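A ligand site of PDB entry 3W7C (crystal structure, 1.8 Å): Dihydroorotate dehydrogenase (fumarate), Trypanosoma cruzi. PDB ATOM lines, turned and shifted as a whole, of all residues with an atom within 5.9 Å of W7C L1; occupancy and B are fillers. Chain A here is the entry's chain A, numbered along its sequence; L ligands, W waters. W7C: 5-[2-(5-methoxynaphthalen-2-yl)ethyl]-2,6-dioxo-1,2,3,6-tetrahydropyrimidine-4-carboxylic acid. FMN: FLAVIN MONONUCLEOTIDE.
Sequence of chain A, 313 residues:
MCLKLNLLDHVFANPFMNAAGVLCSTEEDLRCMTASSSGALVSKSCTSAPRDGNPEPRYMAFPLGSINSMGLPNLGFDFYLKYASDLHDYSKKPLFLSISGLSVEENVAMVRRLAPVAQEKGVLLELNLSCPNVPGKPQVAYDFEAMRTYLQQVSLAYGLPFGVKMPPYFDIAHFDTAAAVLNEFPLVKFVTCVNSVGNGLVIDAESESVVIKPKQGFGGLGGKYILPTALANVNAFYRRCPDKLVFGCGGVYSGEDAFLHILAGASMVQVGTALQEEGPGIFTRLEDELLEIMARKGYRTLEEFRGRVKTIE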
ATOM      1  N   LYS A  44       8.459  36.968   0.781  1.00  0.00           N
ATOM      2  CA  LYS A  44       8.972  35.706   0.306  1.00  0.00           C
ATOM      3  C   LYS A  44      10.361  35.885  -0.312  1.00  0.00           C
ATOM      4  O   LYS A  44      10.573  36.800  -1.084  1.00  0.00           O
ATOM      5  CB  LYS A  44       8.031  35.088  -0.769  1.00  0.00           C
ATOM      6  CG  LYS A  44       8.577  33.887  -1.533  1.00  0.00           C
ATOM      7  CD  LYS A  44       8.742  32.665  -0.691  1.00  0.00           C
ATOM      8  CE  LYS A  44       9.502  31.519  -1.438  1.00  0.00           C
ATOM      9  NZ  LYS A  44       9.685  30.193  -0.681  1.00  0.00           N
ATOM     10  N   SER A  45      11.253  34.956  -0.017  1.00  0.00           N
ATOM     11  CA  SER A  45      12.647  34.941  -0.538  1.00  0.00           C
ATOM     12  C   SER A  45      12.516  34.994  -2.040  1.00  0.00           C
ATOM     13  O   SER A  45      11.752  34.243  -2.639  1.00  0.00           O
ATOM     14  CB  SER A  45      13.404  33.701  -0.144  1.00  0.00           C
ATOM     15  OG  SER A  45      13.769  33.785   1.233  1.00  0.00           O
ATOM     16  N   ARG A  51       9.770  32.674 -10.410  1.00  0.00           N
ATOM     17  CA  ARG A  51       9.904  31.240 -10.467  1.00  0.00           C
ATOM     18  C   ARG A  51       8.534  30.608 -10.126  1.00  0.00           C
ATOM     19  O   ARG A  51       7.821  31.111  -9.230  1.00  0.00           O
ATOM     20  CB  ARG A  51      10.893  30.721  -9.427  1.00  0.00           C
ATOM     21  CG  ARG A  51      12.365  30.981  -9.731  1.00  0.00           C
ATOM     22  CD  ARG A  51      13.240  30.611  -8.538  1.00  0.00           C
ATOM     23  NE  ARG A  51      13.203  29.204  -8.220  1.00  0.00           N
ATOM     24  CZ  ARG A  51      13.936  28.258  -8.801  1.00  0.00           C
ATOM     25  NH1 ARG A  51      14.798  28.532  -9.818  1.00  0.00           N
ATOM     26  NH2 ARG A  51      13.793  27.014  -8.399  1.00  0.00           N
ATOM     27  N   ASN A  54       8.741  24.140  -7.455  1.00  0.00           N
ATOM     28  CA  ASN A  54       8.694  22.704  -7.682  1.00  0.00           C
ATOM     29  C   ASN A  54       7.292  22.166  -7.943  1.00  0.00           C
ATOM     30  O   ASN A  54       6.295  22.843  -7.688  1.00  0.00           O
ATOM     31  CB  ASN A  54       9.321  21.980  -6.454  1.00  0.00           C
ATOM     32  CG  ASN A  54      10.832  22.117  -6.358  1.00  0.00           C
ATOM     33  OD1 ASN A  54      11.518  22.557  -7.322  1.00  0.00           O
ATOM     34  ND2 ASN A  54      11.386  21.734  -5.211  1.00  0.00           N
ATOM     35  N   ASN A  68       8.530  20.583   3.438  1.00  0.00           N
ATOM     36  CA  ASN A  68       8.297  21.300   2.216  1.00  0.00           C
ATOM     37  C   ASN A  68       9.485  21.190   1.281  1.00  0.00           C
ATOM     38  O   ASN A  68      10.658  21.253   1.725  1.00  0.00           O
ATOM     39  CB  ASN A  68       7.962  22.797   2.431  1.00  0.00           C
ATOM     40  CG  ASN A  68       9.194  23.651   2.565  1.00  0.00           C
ATOM     41  OD1 ASN A  68       9.856  24.019   1.554  1.00  0.00           O
ATOM     42  ND2 ASN A  68       9.589  23.958   3.810  1.00  0.00           N
ATOM     43  N   SER A  69       9.167  21.127   0.010  1.00  0.00           N
ATOM     44  CA  SER A  69      10.204  21.389  -1.017  1.00  0.00           C
ATOM     45  C   SER A  69       9.586  22.318  -2.051  1.00  0.00           C
ATOM     46  O   SER A  69       9.353  21.967  -3.204  1.00  0.00           O
ATOM     47  CB  SER A  69      10.710  20.139  -1.600  1.00  0.00           C
ATOM     48  OG  SER A  69      11.768  20.427  -2.553  1.00  0.00           O
ATOM     49  N   MET A  70       9.401  23.551  -1.621  1.00  0.00           N
ATOM     50  CA  MET A  70       8.691  24.479  -2.473  1.00  0.00           C
ATOM     51  C   MET A  70       9.492  24.804  -3.744  1.00  0.00           C
ATOM     52  O   MET A  70       8.943  25.041  -4.830  1.00  0.00           O
ATOM     53  CB  MET A  70       8.455  25.773  -1.756  1.00  0.00           C
ATOM     54  CG  MET A  70       7.675  25.747  -0.496  1.00  0.00           C
ATOM     55  SD  MET A  70       6.056  24.955  -0.606  1.00  0.00           S
ATOM     56  CE  MET A  70       5.099  26.170  -1.449  1.00  0.00           C
ATOM     57  N   GLY A  71      10.800  24.854  -3.608  1.00  0.00           N
ATOM     58  CA  GLY A  71      11.605  25.279  -4.725  1.00  0.00           C
ATOM     59  C   GLY A  71      11.633  26.718  -5.101  1.00  0.00           C
ATOM     60  O   GLY A  71      11.753  27.049  -6.324  1.00  0.00           O
ATOM     61  N   LEU A  72      11.542  27.581  -4.108  1.00  0.00           N
ATOM     62  CA  LEU A  72      11.589  29.043  -4.296  1.00  0.00           C
ATOM     63  C   LEU A  72      10.635  29.595  -5.346  1.00  0.00           C
ATOM     64  O   LEU A  72      10.975  30.444  -6.173  1.00  0.00           O
ATOM     65  CB  LEU A  72      13.029  29.450  -4.578  1.00  0.00           C
ATOM     66  CG  LEU A  72      13.602  30.790  -4.236  1.00  0.00           C
ATOM     67  CD1 LEU A  72      13.224  31.255  -2.857  1.00  0.00           C
ATOM     68  CD2 LEU A  72      15.123  30.700  -4.325  1.00  0.00           C
ATOM     69  N   PRO A  73       9.347  29.251  -5.242  1.00  0.00           N
ATOM     70  CA  PRO A  73       8.403  29.955  -6.087  1.00  0.00           C
ATOM     71  C   PRO A  73       8.251  31.396  -5.623  1.00  0.00           C
ATOM     72  O   PRO A  73       8.144  31.613  -4.427  1.00  0.00           O
ATOM     73  CB  PRO A  73       7.088  29.190  -5.834  1.00  0.00           C
ATOM     74  CG  PRO A  73       7.224  28.624  -4.466  1.00  0.00           C
ATOM     75  CD  PRO A  73       8.718  28.432  -4.220  1.00  0.00           C
ATOM     76  N   SER A 100      17.045  35.477  -1.951  1.00  0.00           N
ATOM     77  CA  SER A 100      17.654  34.172  -2.006  1.00  0.00           C
ATOM     78  C   SER A 100      18.148  33.818  -3.411  1.00  0.00           C
ATOM     79  O   SER A 100      17.706  32.843  -4.056  1.00  0.00           O
ATOM     80  CB  SER A 100      16.665  33.145  -1.421  1.00  0.00           C
ATOM     81  OG  SER A 100      17.215  31.838  -1.481  1.00  0.00           O
ATOM     82  N   LEU A 102      20.390  32.419  -6.460  1.00  0.00           N
ATOM     83  CA  LEU A 102      20.922  31.046  -6.693  1.00  0.00           C
ATOM     84  C   LEU A 102      22.428  31.061  -6.947  1.00  0.00           C
ATOM     85  O   LEU A 102      23.057  29.992  -7.103  1.00  0.00           O
ATOM     86  CB  LEU A 102      20.138  30.299  -7.804  1.00  0.00           C
ATOM     87  CG  LEU A 102      18.621  30.154  -7.422  1.00  0.00           C
ATOM     88  CD1 LEU A 102      17.864  29.100  -8.185  1.00  0.00           C
ATOM     89  CD2 LEU A 102      18.429  29.872  -6.006  1.00  0.00           C
ATOM     90  N   ASN A 128      19.025  35.190   2.664  1.00  0.00           N
ATOM     91  CA  ASN A 128      18.877  33.759   2.931  1.00  0.00           C
ATOM     92  C   ASN A 128      20.104  32.961   2.561  1.00  0.00           C
ATOM     93  O   ASN A 128      20.402  32.793   1.358  1.00  0.00           O
ATOM     94  CB  ASN A 128      17.715  33.203   2.160  1.00  0.00           C
ATOM     95  CG  ASN A 128      17.389  31.738   2.510  1.00  0.00           C
ATOM     96  OD1 ASN A 128      17.875  31.173   3.441  1.00  0.00           O
ATOM     97  ND2 ASN A 128      16.453  31.218   1.803  1.00  0.00           N
ATOM     98  N   SER A 130      20.492  29.790   3.669  1.00  0.00           N
ATOM     99  CA  SER A 130      20.140  28.395   3.728  1.00  0.00           C
ATOM    100  C   SER A 130      19.496  28.057   2.443  1.00  0.00           C
ATOM    101  O   SER A 130      18.277  27.876   2.362  1.00  0.00           O
ATOM    102  CB  SER A 130      19.211  28.057   4.890  1.00  0.00           C
ATOM    103  OG  SER A 130      18.783  26.730   4.762  1.00  0.00           O
ATOM    104  N   CYS A 131      20.268  28.256   1.378  1.00  0.00           N
ATOM    105  CA  CYS A 131      19.867  28.041  -0.016  1.00  0.00           C
ATOM    106  C   CYS A 131      20.926  27.334  -0.853  1.00  0.00           C
ATOM    107  O   CYS A 131      22.119  27.397  -0.555  1.00  0.00           O
ATOM    108  CB  CYS A 131      19.486  29.371  -0.673  1.00  0.00           C
ATOM    109  SG  CYS A 131      20.863  30.540  -0.846  1.00  0.00           S
ATOM    110  N   PRO A 132      20.483  26.658  -1.905  1.00  0.00           N
ATOM    111  CA  PRO A 132      21.362  26.012  -2.867  1.00  0.00           C
ATOM    112  C   PRO A 132      22.386  26.942  -3.522  1.00  0.00           C
ATOM    113  O   PRO A 132      22.136  28.059  -3.728  1.00  0.00           O
ATOM    114  CB  PRO A 132      20.414  25.594  -3.969  1.00  0.00           C
ATOM    115  CG  PRO A 132      19.072  25.498  -3.347  1.00  0.00           C
ATOM    116  CD  PRO A 132      19.134  26.082  -1.973  1.00  0.00           C
ATOM    117  N   LYS A 165      19.559  34.783   7.255  1.00  0.00           N
ATOM    118  CA  LYS A 165      18.803  33.585   7.623  1.00  0.00           C
ATOM    119  C   LYS A 165      19.656  32.336   7.536  1.00  0.00           C
ATOM    120  O   LYS A 165      20.208  32.021   6.495  1.00  0.00           O
ATOM    121  CB  LYS A 165      17.601  33.482   6.686  1.00  0.00           C
ATOM    122  CG  LYS A 165      16.716  32.276   6.968  1.00  0.00           C
ATOM    123  CD  LYS A 165      15.817  32.505   8.167  1.00  0.00           C
ATOM    124  CE  LYS A 165      14.663  31.497   8.293  1.00  0.00           C
ATOM    125  NZ  LYS A 165      13.587  31.665   7.299  1.00  0.00           N
ATOM    126  N   ASN A 195      16.296  28.372   9.637  1.00  0.00           N
ATOM    127  CA  ASN A 195      15.550  27.816   8.498  1.00  0.00           C
ATOM    128  C   ASN A 195      15.156  26.354   8.826  1.00  0.00           C
ATOM    129  O   ASN A 195      15.474  25.842   9.863  1.00  0.00           O
ATOM    130  CB  ASN A 195      16.422  27.887   7.234  1.00  0.00           C
ATOM    131  CG  ASN A 195      15.606  28.118   5.985  1.00  0.00           C
ATOM    132  OD1 ASN A 195      14.686  27.490   5.748  1.00  0.00           O
ATOM    133  ND2 ASN A 195      16.013  29.080   5.215  1.00  0.00           N
ATOM    134  N   SER A 196      14.455  25.714   7.898  1.00  0.00           N
ATOM    135  CA  SER A 196      13.943  24.365   8.103  1.00  0.00           C
ATOM    136  C   SER A 196      15.046  23.322   8.247  1.00  0.00           C
ATOM    137  O   SER A 196      16.077  23.378   7.570  1.00  0.00           O
ATOM    138  CB  SER A 196      12.999  23.974   6.970  1.00  0.00           C
ATOM    139  OG  SER A 196      13.603  24.200   5.700  1.00  0.00           O
ATOM    140  N   PRO A 214       8.541  16.528  -4.956  1.00  0.00           N
ATOM    141  CA  PRO A 214       9.912  16.760  -5.338  1.00  0.00           C
ATOM    142  C   PRO A 214      10.919  15.934  -4.537  1.00  0.00           C
ATOM    143  O   PRO A 214      10.603  15.478  -3.432  1.00  0.00           O
ATOM    144  CB  PRO A 214      10.122  18.258  -5.034  1.00  0.00           C
ATOM    145  CG  PRO A 214       8.734  18.800  -4.983  1.00  0.00           C
ATOM    146  CD  PRO A 214       7.917  17.734  -4.424  1.00  0.00           C
ATOM    147  N   LYS A 215      12.120  15.702  -5.127  1.00  0.00           N
ATOM    148  CA  LYS A 215      13.269  15.093  -4.458  1.00  0.00           C
ATOM    149  C   LYS A 215      12.869  13.786  -3.700  1.00  0.00           C
ATOM    150  O   LYS A 215      13.381  13.472  -2.598  1.00  0.00           O
ATOM    151  CB  LYS A 215      14.023  16.168  -3.599  1.00  0.00           C
ATOM    152  CG  LYS A 215      15.251  16.887  -4.237  1.00  0.00           C
ATOM    153  CD  LYS A 215      15.286  16.917  -5.748  1.00  0.00           C
ATOM    154  CE  LYS A 215      16.331  17.864  -6.330  1.00  0.00           C
ATOM    155  NZ  LYS A 215      16.159  19.132  -5.582  1.00  0.00           N
ATOM    156  N   GLY A 220      12.405  20.086   3.702  1.00  0.00           N
ATOM    157  CA  GLY A 220      12.749  20.706   4.953  1.00  0.00           C
ATOM    158  C   GLY A 220      11.616  20.636   5.974  1.00  0.00           C
ATOM    159  O   GLY A 220      10.448  20.861   5.672  1.00  0.00           O
HETATM  160  OAB W7C L   1      11.329  27.701  -1.288  1.00  0.00           O
HETATM  161  CAQ W7C L   1      11.810  26.819  -0.552  1.00  0.00           C
HETATM  162  OAE W7C L   1      11.697  25.629  -0.846  1.00  0.00           O
HETATM  163  CAT W7C L   1      12.398  27.092   0.737  1.00  0.00           C
HETATM  164  NAN W7C L   1      11.868  26.263   1.777  1.00  0.00           N
HETATM  165  CAV W7C L   1      12.393  26.393   3.059  1.00  0.00           C
HETATM  166  OAC W7C L   1      11.976  25.687   3.973  1.00  0.00           O
HETATM  167  NAO W7C L   1      13.426  27.275   3.275  1.00  0.00           N
HETATM  168  CAW W7C L   1      14.021  28.054   2.240  1.00  0.00           C
HETATM  169  OAD W7C L   1      14.918  28.827   2.561  1.00  0.00           O
HETATM  170  CAU W7C L   1      13.485  27.952   0.968  1.00  0.00           C
HETATM  171  CAM W7C L   1      13.999  28.643  -0.100  1.00  0.00           C
HETATM  172  CAL W7C L   1      15.480  28.240  -0.409  1.00  0.00           C
HETATM  173  CAR W7C L   1      15.430  27.121  -1.324  1.00  0.00           C
HETATM  174  CAK W7C L   1      15.480  27.209  -2.717  1.00  0.00           C
HETATM  175  CAH W7C L   1      15.287  25.855  -0.766  1.00  0.00           C
HETATM  176  CAJ W7C L   1      15.178  24.712  -1.531  1.00  0.00           C
HETATM  177  CAY W7C L   1      15.192  24.795  -2.907  1.00  0.00           C
HETATM  178  CAX W7C L   1      15.426  26.044  -3.513  1.00  0.00           C
HETATM  179  CAI W7C L   1      15.460  26.071  -4.910  1.00  0.00           C
HETATM  180  CAF W7C L   1      15.285  24.902  -5.657  1.00  0.00           C
HETATM  181  CAG W7C L   1      15.132  23.655  -5.046  1.00  0.00           C
HETATM  182  CAS W7C L   1      15.094  23.610  -3.662  1.00  0.00           C
HETATM  183  OAP W7C L   1      14.984  22.452  -2.885  1.00  0.00           O
HETATM  184  CAA W7C L   1      14.895  21.226  -3.539  1.00  0.00           C
HETATM  185  N1  FMN L   2      12.757  30.300   4.630  1.00  0.00           N
HETATM  186  C2  FMN L   2      13.361  31.238   3.915  1.00  0.00           C
HETATM  187  O2  FMN L   2      14.278  31.851   4.468  1.00  0.00           O
HETATM  188  N3  FMN L   2      12.902  31.621   2.686  1.00  0.00           N
HETATM  189  C4  FMN L   2      11.822  31.082   2.093  1.00  0.00           C
HETATM  190  O4  FMN L   2      11.309  31.459   0.981  1.00  0.00           O
HETATM  191  C4A FMN L   2      11.100  30.086   2.822  1.00  0.00           C
HETATM  192  N5  FMN L   2      10.027  29.439   2.307  1.00  0.00           N
HETATM  193  C5A FMN L   2       9.258  28.596   3.077  1.00  0.00           C
HETATM  194  C6  FMN L   2       8.087  28.061   2.598  1.00  0.00           C
HETATM  195  C7  FMN L   2       7.344  27.131   3.350  1.00  0.00           C
HETATM  196  C7M FMN L   2       6.062  26.567   2.842  1.00  0.00           C
HETATM  197  C8  FMN L   2       7.792  26.753   4.699  1.00  0.00           C
HETATM  198  C8M FMN L   2       7.036  25.776   5.528  1.00  0.00           C
HETATM  199  C9  FMN L   2       9.000  27.260   5.177  1.00  0.00           C
HETATM  200  C9A FMN L   2       9.734  28.193   4.407  1.00  0.00           C
HETATM  201  N10 FMN L   2      10.931  28.766   4.857  1.00  0.00           N
HETATM  202  C10 FMN L   2      11.632  29.727   4.143  1.00  0.00           C
HETATM  203  C1' FMN L   2      11.427  28.451   6.160  1.00  0.00           C
HETATM  204  C2' FMN L   2      10.716  29.205   7.273  1.00  0.00           C
HETATM  205  O2' FMN L   2      10.959  30.580   7.095  1.00  0.00           O
HETATM  206  C3' FMN L   2      11.198  28.752   8.648  1.00  0.00           C
HETATM  207  O3' FMN L   2      12.608  29.079   8.842  1.00  0.00           O
HETATM  208  C4' FMN L   2      10.914  27.231   8.932  1.00  0.00           C
HETATM  209  O4' FMN L   2       9.678  26.793   8.414  1.00  0.00           O
HETATM  210  C5' FMN L   2      10.955  26.940  10.434  1.00  0.00           C
HETATM  211  O5' FMN L   2       9.978  27.633  11.204  1.00  0.00           O
HETATM  212  P   FMN L   2       8.598  26.954  11.722  1.00  0.00           P
HETATM  213  O1P FMN L   2       7.810  28.076  12.331  1.00  0.00           O
HETATM  214  O2P FMN L   2       8.999  25.782  12.557  1.00  0.00           O
HETATM  215  O3P FMN L   2       7.946  26.460  10.446  1.00  0.00           O
HETATM  216  O   HOH W   1      12.683  23.404   0.778  1.00  0.00           O
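OD1 of Asn 195 is in hydrogen-bond range of NAO of W7C L1, at 2.8 Å.
The side-chain hydroxyl of Ser 196 sits at hydrogen-bond distance from an oxygen (OAC) of W7C L1 (2.8 Å).
An oxygen (OAB) of W7C L1 sits at hydrogen-bond distance from the backbone NH (N) of Leu 72 (2.8 Å).
The side-chain amide nitrogen (ND2) of Asn 128 sits at hydrogen-bond distance from an oxygen (OAD) of W7C L1, 2.9 Å away.
ND2 of Asn 68 sits at hydrogen-bond distance from OAC of W7C L1 (3.0 Å).
OAE of W7C L1 lies within hydrogen-bond range of N of Gly 71 (3.0 Å).
NZ of Lys 44 is in salt-bridge range of OAB of W7C L1, at 3.0 Å.
An oxygen (OAE) of W7C L1 is in hydrogen-bond range of the backbone NH of Met 70, at 3.2 Å.
The side-chain amide nitrogen (ND2) of Asn 195 lies within hydrogen-bond range of an oxygen (O2) of FMN L2 (3.4 Å).
An oxygen (O2) of FMN L2 lies within hydrogen-bond range of the side-chain amide nitrogen (ND2) of Asn 128 (3.5 Å).
NZ of Lys 44 lies within hydrogen-bond range of O4 of FMN L2 (2.6 Å).
The side-chain hydroxyl (OG) of Ser 45 is in hydrogen-bond range of a nitrogen (N3) of FMN L2 (2.7 Å).
An oxygen (O2') of FMN L2 lies within hydrogen-bond range of the side-chain amino group (NZ) of Lys 165 (2.9 Å).
N1 of FMN L2 lies close to NAO of W7C L1 (3.4 Å).
The side-chain amide oxygen of Asn 128 is in hydrogen-bond range of the side-chain amide nitrogen of Asn 195, 3.3 Å away.
The guanidinium group of Arg 51 lies close to the backbone carbonyl oxygen of Leu 72, 3.3 Å away.
The side-chain amide oxygen (OD1) of Asn 128 sits at hydrogen-bond distance from the backbone NH (N) of Ser 130, 3.0 Å away.
The side-chain amide oxygen (OD1) of Asn 68 sits at hydrogen-bond distance from the backbone NH (N) of Met 70, at 3.2 Å.
The backbone carbonyl oxygen (O) of Asn 68 sits at hydrogen-bond distance from the backbone NH (N) of Gly 220 (2.9 Å).
O of Gly 71 sits at hydrogen-bond distance from NH2 of Arg 51 (2.9 Å).
O of Met 70 sits at hydrogen-bond distance from N of Asn 54, 2.8 Å away.
ND2 of Asn 54 is in hydrogen-bond range of O of Ser 69, at 2.9 Å.
Water W1 lies within hydrogen-bond range of OAE of W7C L1 (2.9 Å) and OD1 of Asn 68 (3.0 Å).
An oxygen (OAD) of W7C L1 sits close to the backbone carbonyl oxygen (O) of Ser 130 (3.5 Å).
Arg 51 touches W7C L1.
ND2 of Asn 54 touches CAA of W7C L1, 3.9 Å away.
Ser 69 touches W7C L1 (OG to CAA, 3.4 Å).
Pro 73 touches W7C L1.
CG of Pro 132 touches CAX of W7C L1 (3.7 Å).
Lys 215 touches W7C L1 (NZ to CAA, 3.2 Å).
Hydrophobic or aromatic side chains within 4 Å of W7C L1: Met 70, Leu 72, Pro 73 and Pro 132.
15 residues have an atom within 4 Å of W7C L1: Lys 44, Arg 51, Asn 54, Asn 68, Ser 69, Met 70, Gly 71, Leu 72, Pro 73, Asn 128, Ser 130, Pro 132, Asn 195, Ser 196 and Lys 215.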
